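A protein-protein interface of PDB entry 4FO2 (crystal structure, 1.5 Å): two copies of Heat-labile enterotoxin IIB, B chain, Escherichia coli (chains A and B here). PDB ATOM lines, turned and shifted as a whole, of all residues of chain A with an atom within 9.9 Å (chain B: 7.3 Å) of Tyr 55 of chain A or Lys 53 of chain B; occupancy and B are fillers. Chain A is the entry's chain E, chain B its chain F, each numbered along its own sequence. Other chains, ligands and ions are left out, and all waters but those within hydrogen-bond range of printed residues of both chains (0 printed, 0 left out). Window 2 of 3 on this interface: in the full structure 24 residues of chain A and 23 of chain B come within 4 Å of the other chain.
Tyr 55 of chain A touches just these residues of chain B: Arg 51, Ala 52 and Lys 53.
Printed residues of chain A within 4 Å of Ala 52 of chain B: Tyr 55 (3.4 Å).
No residue of chain A comes within 4 Å of Asp 54 of chain B.
Printed residues of chain A within 4 Å of Arg 51 of chain B: Tyr 55, Pro 56 and Met 60.
Printed residues of chain B within 4 Å of Pro 56 of chain A: Arg 51 (3.4 Å).
Printed residues of chain B within 4 Å of Met 60 of chain A: Arg 51.
Printed residues of chain A within 4 Å of Arg 65 of chain B: Val 59 (3.5 Å).
Printed residues of chain B within 4 Å of Val 59 of chain A: Arg 65.
Thr 61 of chain B touches none of the printed residues of chain A.
Asp 54 of chain A touches none of the printed residues of chain B.
The nearest residue of chain A that does not touch Lys 53 of chain B is Asp 54 of chain A (6.4 Å).
N of Lys 53 of chain B lies within hydrogen-bond range of OH of Tyr 55 of chain A (3.4 Å).
OH of Tyr 55 of chain A lies within hydrogen-bond range of N of Ala 52 of chain B, at 3.4 Å.
The side-chain amide nitrogen of Asn 58 of chain B is in hydrogen-bond range of the backbone carbonyl oxygen of Lys 53 of chain B (3.1 Å).
The backbone NH (N) of Tyr 55 of chain A lies close to the side-chain amide oxygen (OD1) of Asn 58 of chain A.
Tyr 55 of chain A touches Arg 51 of chain B, but with the chains exchanged Arg 51 of chain A does not touch Tyr 55 of chain B (21.4 Å).
Tyr 55 of chain A touches Ala 52 of chain B, but with the chains exchanged Ala 52 of chain A does not touch Tyr 55 of chain B (18.0 Å).
Tyr 55 of chain A touches Lys 53 of chain B, but with the chains exchanged Lys 53 of chain A does not touch Tyr 55 of chain B (15.7 Å).
Of the 6 pairs that touch across the chains among the printed residues, none has its exchanged pair printed and touching as well.
Arg 51 of chain B touches Tyr 55 of chain A (CG to OH, 3.2 Å).
Pro 56 of chain A touches Arg 51 of chain B.
Val 59 of chain A touches Arg 65 of chain B.
Met 60 of chain A touches Arg 51 of chain B (CE to NH1, 3.6 Å).
Of the 11 printed residues of chain A, 4 touch a printed residue of chain B.
Of the 11 printed residues of chain B, 4 touch a printed residue of chain A.
Among the printed residues, 6 pairs touch across the chains.
Among the printed residues, no Asp or Glu carboxylate lies within 4 Å of a Lys or Arg side-chain nitrogen of the other chain.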
ATOM      1  N   ARG A  51      14.846  26.833   9.732  1.00  0.00           N
ATOM      2  CA  ARG A  51      13.787  26.737   8.674  1.00  0.00           C
ATOM      3  C   ARG A  51      13.742  28.056   7.943  1.00  0.00           C
ATOM      4  O   ARG A  51      14.325  29.009   8.434  1.00  0.00           O
ATOM      5  CB  ARG A  51      12.410  26.403   9.203  1.00  0.00           C
ATOM      6  CG  ARG A  51      11.956  27.279  10.410  1.00  0.00           C
ATOM      7  CD  ARG A  51      10.483  27.040  10.795  1.00  0.00           C
ATOM      8  NE  ARG A  51       9.914  28.238  11.416  1.00  0.00           N
ATOM      9  CZ  ARG A  51       9.359  28.373  12.622  1.00  0.00           C
ATOM     10  NH1 ARG A  51       9.201  27.365  13.517  1.00  0.00           N
ATOM     11  NH2 ARG A  51       8.943  29.595  12.943  1.00  0.00           N
ATOM     12  N   ALA A  52      13.237  28.043   6.726  1.00  0.00           N
ATOM     13  CA  ALA A  52      13.216  29.296   5.968  1.00  0.00           C
ATOM     14  C   ALA A  52      11.947  29.309   5.182  1.00  0.00           C
ATOM     15  O   ALA A  52      11.535  28.260   4.660  1.00  0.00           O
ATOM     16  CB  ALA A  52      14.412  29.367   5.018  1.00  0.00           C
ATOM     17  N   LYS A  53      11.310  30.469   4.993  1.00  0.00           N
ATOM     18  CA  LYS A  53      10.101  30.333   4.119  1.00  0.00           C
ATOM     19  C   LYS A  53      10.317  30.386   2.629  1.00  0.00           C
ATOM     20  O   LYS A  53       9.531  29.796   1.877  1.00  0.00           O
ATOM     21  CB  LYS A  53       8.945  31.208   4.536  1.00  0.00           C
ATOM     22  CG  LYS A  53       9.243  32.609   4.506  1.00  0.00           C
ATOM     23  CD  LYS A  53       8.039  33.360   5.178  1.00  0.00           C
ATOM     24  CE  LYS A  53       8.617  34.502   6.022  1.00  0.00           C
ATOM     25  NZ  LYS A  53       9.968  34.798   5.425  1.00  0.00           N
ATOM     26  N   ASP A  54      11.442  30.962   2.192  1.00  0.00           N
ATOM     27  CA  ASP A  54      11.639  31.323   0.817  1.00  0.00           C
ATOM     28  C   ASP A  54      12.836  30.618   0.205  1.00  0.00           C
ATOM     29  O   ASP A  54      13.736  30.210   0.947  1.00  0.00           O
ATOM     30  CB  ASP A  54      12.029  32.794   0.770  1.00  0.00           C
ATOM     31  CG  ASP A  54      10.949  33.704   1.267  1.00  0.00           C
ATOM     32  OD1 ASP A  54       9.749  33.449   0.974  1.00  0.00           O
ATOM     33  OD2 ASP A  54      11.332  34.695   1.916  1.00  0.00           O
ATOM     34  N   TYR A  55      12.856  30.560  -1.131  1.00  0.00           N
ATOM     35  CA  TYR A  55      14.014  30.177  -1.912  1.00  0.00           C
ATOM     36  C   TYR A  55      15.032  31.335  -1.825  1.00  0.00           C
ATOM     37  O   TYR A  55      14.621  32.502  -1.864  1.00  0.00           O
ATOM     38  CB  TYR A  55      13.531  29.896  -3.356  1.00  0.00           C
ATOM     39  CG  TYR A  55      14.663  29.571  -4.279  1.00  0.00           C
ATOM     40  CD1 TYR A  55      15.379  30.572  -4.891  1.00  0.00           C
ATOM     41  CD2 TYR A  55      15.030  28.247  -4.524  1.00  0.00           C
ATOM     42  CE1 TYR A  55      16.432  30.312  -5.727  1.00  0.00           C
ATOM     43  CE2 TYR A  55      16.115  27.976  -5.381  1.00  0.00           C
ATOM     44  CZ  TYR A  55      16.827  28.983  -5.964  1.00  0.00           C
ATOM     45  OH  TYR A  55      17.895  28.720  -6.793  1.00  0.00           O
ATOM     46  N   PRO A  56      16.353  31.035  -1.689  1.00  0.00           N
ATOM     47  CA  PRO A  56      16.909  29.671  -1.732  1.00  0.00           C
ATOM     48  C   PRO A  56      17.113  28.984  -0.434  1.00  0.00           C
ATOM     49  O   PRO A  56      17.470  27.808  -0.461  1.00  0.00           O
ATOM     50  CB  PRO A  56      18.267  29.930  -2.365  1.00  0.00           C
ATOM     51  CG  PRO A  56      18.690  31.288  -1.740  1.00  0.00           C
ATOM     52  CD  PRO A  56      17.415  32.054  -1.818  1.00  0.00           C
ATOM     53  N   ASP A  57      16.988  29.656   0.717  1.00  0.00           N
ATOM     54  CA  ASP A  57      17.343  28.989   1.996  1.00  0.00           C
ATOM     55  C   ASP A  57      16.449  27.795   2.256  1.00  0.00           C
ATOM     56  O   ASP A  57      16.896  26.873   2.954  1.00  0.00           O
ATOM     57  CB  ASP A  57      17.365  29.976   3.205  1.00  0.00           C
ATOM     58  CG  ASP A  57      18.572  30.916   3.223  1.00  0.00           C
ATOM     59  OD1 ASP A  57      19.628  30.622   2.601  1.00  0.00           O
ATOM     60  OD2 ASP A  57      18.417  31.939   3.938  1.00  0.00           O
ATOM     61  N   ASN A  58      15.236  27.759   1.665  1.00  0.00           N
ATOM     62  CA  ASN A  58      14.398  26.614   2.018  1.00  0.00           C
ATOM     63  C   ASN A  58      14.813  25.360   1.277  1.00  0.00           C
ATOM     64  O   ASN A  58      14.369  24.320   1.653  1.00  0.00           O
ATOM     65  CB  ASN A  58      12.916  26.861   1.809  1.00  0.00           C
ATOM     66  CG  ASN A  58      12.560  27.174   0.398  1.00  0.00           C
ATOM     67  OD1 ASN A  58      13.331  27.143  -0.597  1.00  0.00           O
ATOM     68  ND2 ASN A  58      11.256  27.606   0.275  1.00  0.00           N
ATOM     69  N   VAL A  59      15.707  25.471   0.297  1.00  0.00           N
ATOM     70  CA  VAL A  59      16.337  24.294  -0.327  1.00  0.00           C
ATOM     71  C   VAL A  59      17.246  23.747   0.749  1.00  0.00           C
ATOM     72  O   VAL A  59      17.163  22.539   1.043  1.00  0.00           O
ATOM     73  CB  VAL A  59      17.135  24.689  -1.561  1.00  0.00           C
ATOM     74  CG1 VAL A  59      18.060  23.475  -2.003  1.00  0.00           C
ATOM     75  CG2 VAL A  59      16.093  25.079  -2.702  1.00  0.00           C
ATOM     76  N   MET A  60      18.121  24.579   1.301  1.00  0.00           N
ATOM     77  CA  MET A  60      19.067  24.112   2.248  1.00  0.00           C
ATOM     78  C   MET A  60      18.421  23.580   3.542  1.00  0.00           C
ATOM     79  O   MET A  60      18.872  22.584   4.095  1.00  0.00           O
ATOM     80  CB  MET A  60      20.191  25.137   2.546  1.00  0.00           C
ATOM     81  CG  MET A  60      21.298  25.185   1.433  1.00  0.00           C
ATOM     82  SD  MET A  60      20.747  25.952  -0.058  1.00  0.00           S
ATOM     83  CE  MET A  60      20.924  27.656   0.402  1.00  0.00           C
ATOM     84  N   THR A  61      17.411  24.278   4.086  1.00  0.00           N
ATOM     85  CA  THR A  61      16.781  23.813   5.313  1.00  0.00           C
ATOM     86  C   THR A  61      16.088  22.449   5.069  1.00  0.00           C
ATOM     87  O   THR A  61      16.115  21.594   5.970  1.00  0.00           O
ATOM     88  CB  THR A  61      15.852  24.847   5.905  1.00  0.00           C
ATOM     89  OG1 THR A  61      14.836  25.142   4.962  1.00  0.00           O
ATOM     90  CG2 THR A  61      16.657  26.128   6.255  1.00  0.00           C
ATOM     91  N   SER B  50      24.259  22.431  -7.953  1.00  0.00           N
ATOM     92  CA  SER B  50      23.486  23.623  -8.445  1.00  0.00           C
ATOM     93  C   SER B  50      22.145  23.775  -7.852  1.00  0.00           C
ATOM     94  O   SER B  50      21.590  22.750  -7.356  1.00  0.00           O
ATOM     95  CB  SER B  50      23.327  23.668  -9.970  1.00  0.00           C
ATOM     96  OG  SER B  50      24.648  23.948 -10.439  1.00  0.00           O
ATOM     97  N   ARG B  51      21.624  25.000  -7.841  1.00  0.00           N
ATOM     98  CA  ARG B  51      20.359  25.290  -7.229  1.00  0.00           C
ATOM     99  C   ARG B  51      19.590  26.007  -8.356  1.00  0.00           C
ATOM    100  O   ARG B  51      20.196  26.736  -9.151  1.00  0.00           O
ATOM    101  CB  ARG B  51      20.702  26.385  -6.123  1.00  0.00           C
ATOM    102  CG  ARG B  51      19.767  26.741  -5.194  1.00  0.00           C
ATOM    103  CD  ARG B  51      20.450  27.587  -4.099  1.00  0.00           C
ATOM    104  NE  ARG B  51      20.845  28.969  -4.409  1.00  0.00           N
ATOM    105  CZ  ARG B  51      21.654  29.715  -3.671  1.00  0.00           C
ATOM    106  NH1 ARG B  51      22.262  29.210  -2.572  1.00  0.00           N
ATOM    107  NH2 ARG B  51      21.887  30.968  -4.036  1.00  0.00           N
ATOM    108  N   ALA B  52      18.294  25.771  -8.460  1.00  0.00           N
ATOM    109  CA  ALA B  52      17.482  26.554  -9.422  1.00  0.00           C
ATOM    110  C   ALA B  52      16.060  26.688  -8.922  1.00  0.00           C
ATOM    111  O   ALA B  52      15.426  25.700  -8.563  1.00  0.00           O
ATOM    112  CB  ALA B  52      17.520  25.961 -10.809  1.00  0.00           C
ATOM    113  N   LYS B  53      15.467  27.877  -9.068  1.00  0.00           N
ATOM    114  CA  LYS B  53      14.149  28.153  -8.540  1.00  0.00           C
ATOM    115  C   LYS B  53      13.070  27.605  -9.506  1.00  0.00           C
ATOM    116  O   LYS B  53      12.000  27.024  -9.101  1.00  0.00           O
ATOM    117  CB  LYS B  53      14.056  29.692  -8.519  1.00  0.00           C
ATOM    118  CG  LYS B  53      12.790  30.369  -7.922  1.00  0.00           C
ATOM    119  CD  LYS B  53      12.062  29.620  -6.837  1.00  0.00           C
ATOM    120  CE  LYS B  53      11.322  30.698  -5.993  1.00  0.00           C
ATOM    121  NZ  LYS B  53      10.004  31.114  -6.518  1.00  0.00           N
ATOM    122  N   ASP B  54      13.381  27.775 -10.775  1.00  0.00           N
ATOM    123  CA  ASP B  54      12.368  27.580 -11.810  1.00  0.00           C
ATOM    124  C   ASP B  54      12.505  26.287 -12.588  1.00  0.00           C
ATOM    125  O   ASP B  54      13.550  25.658 -12.582  1.00  0.00           O
ATOM    126  CB  ASP B  54      12.371  28.782 -12.738  1.00  0.00           C
ATOM    127  CG  ASP B  54      11.865  30.051 -12.032  1.00  0.00           C
ATOM    128  OD1 ASP B  54      12.253  31.097 -12.504  1.00  0.00           O
ATOM    129  OD2 ASP B  54      11.109  29.978 -11.022  1.00  0.00           O
ATOM    130  N   TYR B  55      11.391  25.891 -13.179  1.00  0.00           N
ATOM    131  CA  TYR B  55      11.337  24.745 -14.088  1.00  0.00           C
ATOM    132  C   TYR B  55      12.057  25.099 -15.445  1.00  0.00           C
ATOM    133  O   TYR B  55      11.968  26.270 -15.941  1.00  0.00           O
ATOM    134  CB  TYR B  55       9.897  24.358 -14.333  1.00  0.00           C
ATOM    135  CG  TYR B  55       9.725  23.259 -15.323  1.00  0.00           C
ATOM    136  CD1 TYR B  55       9.636  21.923 -14.869  1.00  0.00           C
ATOM    137  CD2 TYR B  55       9.482  23.506 -16.703  1.00  0.00           C
ATOM    138  CE1 TYR B  55       9.454  20.889 -15.772  1.00  0.00           C
ATOM    139  CE2 TYR B  55       9.278  22.449 -17.608  1.00  0.00           C
ATOM    140  CZ  TYR B  55       9.221  21.148 -17.127  1.00  0.00           C
ATOM    141  OH  TYR B  55       9.050  20.090 -18.044  1.00  0.00           O
ATOM    142  N   ASP B  57      15.093  23.378 -14.525  1.00  0.00           N
ATOM    143  CA  ASP B  57      16.275  23.061 -13.703  1.00  0.00           C
ATOM    144  C   ASP B  57      15.994  22.732 -12.295  1.00  0.00           C
ATOM    145  O   ASP B  57      16.789  22.027 -11.691  1.00  0.00           O
ATOM    146  CB  ASP B  57      17.326  24.173 -13.849  1.00  0.00           C
ATOM    147  CG  ASP B  57      18.076  24.097 -15.159  1.00  0.00           C
ATOM    148  OD1 ASP B  57      17.890  23.117 -15.937  1.00  0.00           O
ATOM    149  OD2 ASP B  57      18.828  25.060 -15.434  1.00  0.00           O
ATOM    150  N   ASN B  58      14.880  23.172 -11.746  1.00  0.00           N
ATOM    151  CA  ASN B  58      14.510  22.783 -10.413  1.00  0.00           C
ATOM    152  C   ASN B  58      14.312  21.280 -10.242  1.00  0.00           C
ATOM    153  O   ASN B  58      14.376  20.807  -9.087  1.00  0.00           O
ATOM    154  CB  ASN B  58      13.297  23.580  -9.873  1.00  0.00           C
ATOM    155  CG  ASN B  58      12.052  23.422 -10.677  1.00  0.00           C
ATOM    156  OD1 ASN B  58      11.849  22.560 -11.530  1.00  0.00           O
ATOM    157  ND2 ASN B  58      11.028  24.269 -10.215  1.00  0.00           N
ATOM    158  N   VAL B  59      13.936  20.604 -11.374  1.00  0.00           N
ATOM    159  CA  VAL B  59      13.791  19.161 -11.365  1.00  0.00           C
ATOM    160  C   VAL B  59      15.191  18.557 -11.302  1.00  0.00           C
ATOM    161  O   VAL B  59      15.508  17.748 -10.350  1.00  0.00           O
ATOM    162  CB  VAL B  59      13.097  18.680 -12.656  1.00  0.00           C
ATOM    163  CG1 VAL B  59      13.167  17.160 -12.745  1.00  0.00           C
ATOM    164  CG2 VAL B  59      11.626  19.179 -12.523  1.00  0.00           C
ATOM    165  N   THR B  61      18.139  19.802 -10.476  1.00  0.00           N
ATOM    166  CA  THR B  61      18.947  20.104  -9.279  1.00  0.00           C
ATOM    167  C   THR B  61      18.441  19.346  -8.083  1.00  0.00           C
ATOM    168  O   THR B  61      19.209  18.840  -7.294  1.00  0.00           O
ATOM    169  CB  THR B  61      18.974  21.622  -8.966  1.00  0.00           C
ATOM    170  OG1 THR B  61      17.618  22.109  -8.890  1.00  0.00           O
ATOM    171  CG2 THR B  61      19.692  22.346 -10.106  1.00  0.00           C
ATOM    172  N   ARG B  65      20.663  16.579  -5.860  1.00  0.00           N
ATOM    173  CA  ARG B  65      20.690  16.438  -4.408  1.00  0.00           C
ATOM    174  C   ARG B  65      20.347  15.026  -3.990  1.00  0.00           C
ATOM    175  O   ARG B  65      21.071  14.498  -3.176  1.00  0.00           O
ATOM    176  CB  ARG B  65      19.791  17.399  -3.640  1.00  0.00           C
ATOM    177  CG  ARG B  65      20.335  18.869  -3.844  1.00  0.00           C
ATOM    178  CD  ARG B  65      19.393  19.731  -3.029  1.00  0.00           C
ATOM    179  NE  ARG B  65      17.990  19.833  -3.495  1.00  0.00           N
ATOM    180  CZ  ARG B  65      17.516  20.755  -4.353  1.00  0.00           C
ATOM    181  NH1 ARG B  65      18.353  21.606  -4.965  1.00  0.00           N
ATOM    182  NH2 ARG B  65      16.195  20.787  -4.625  1.00  0.00           N
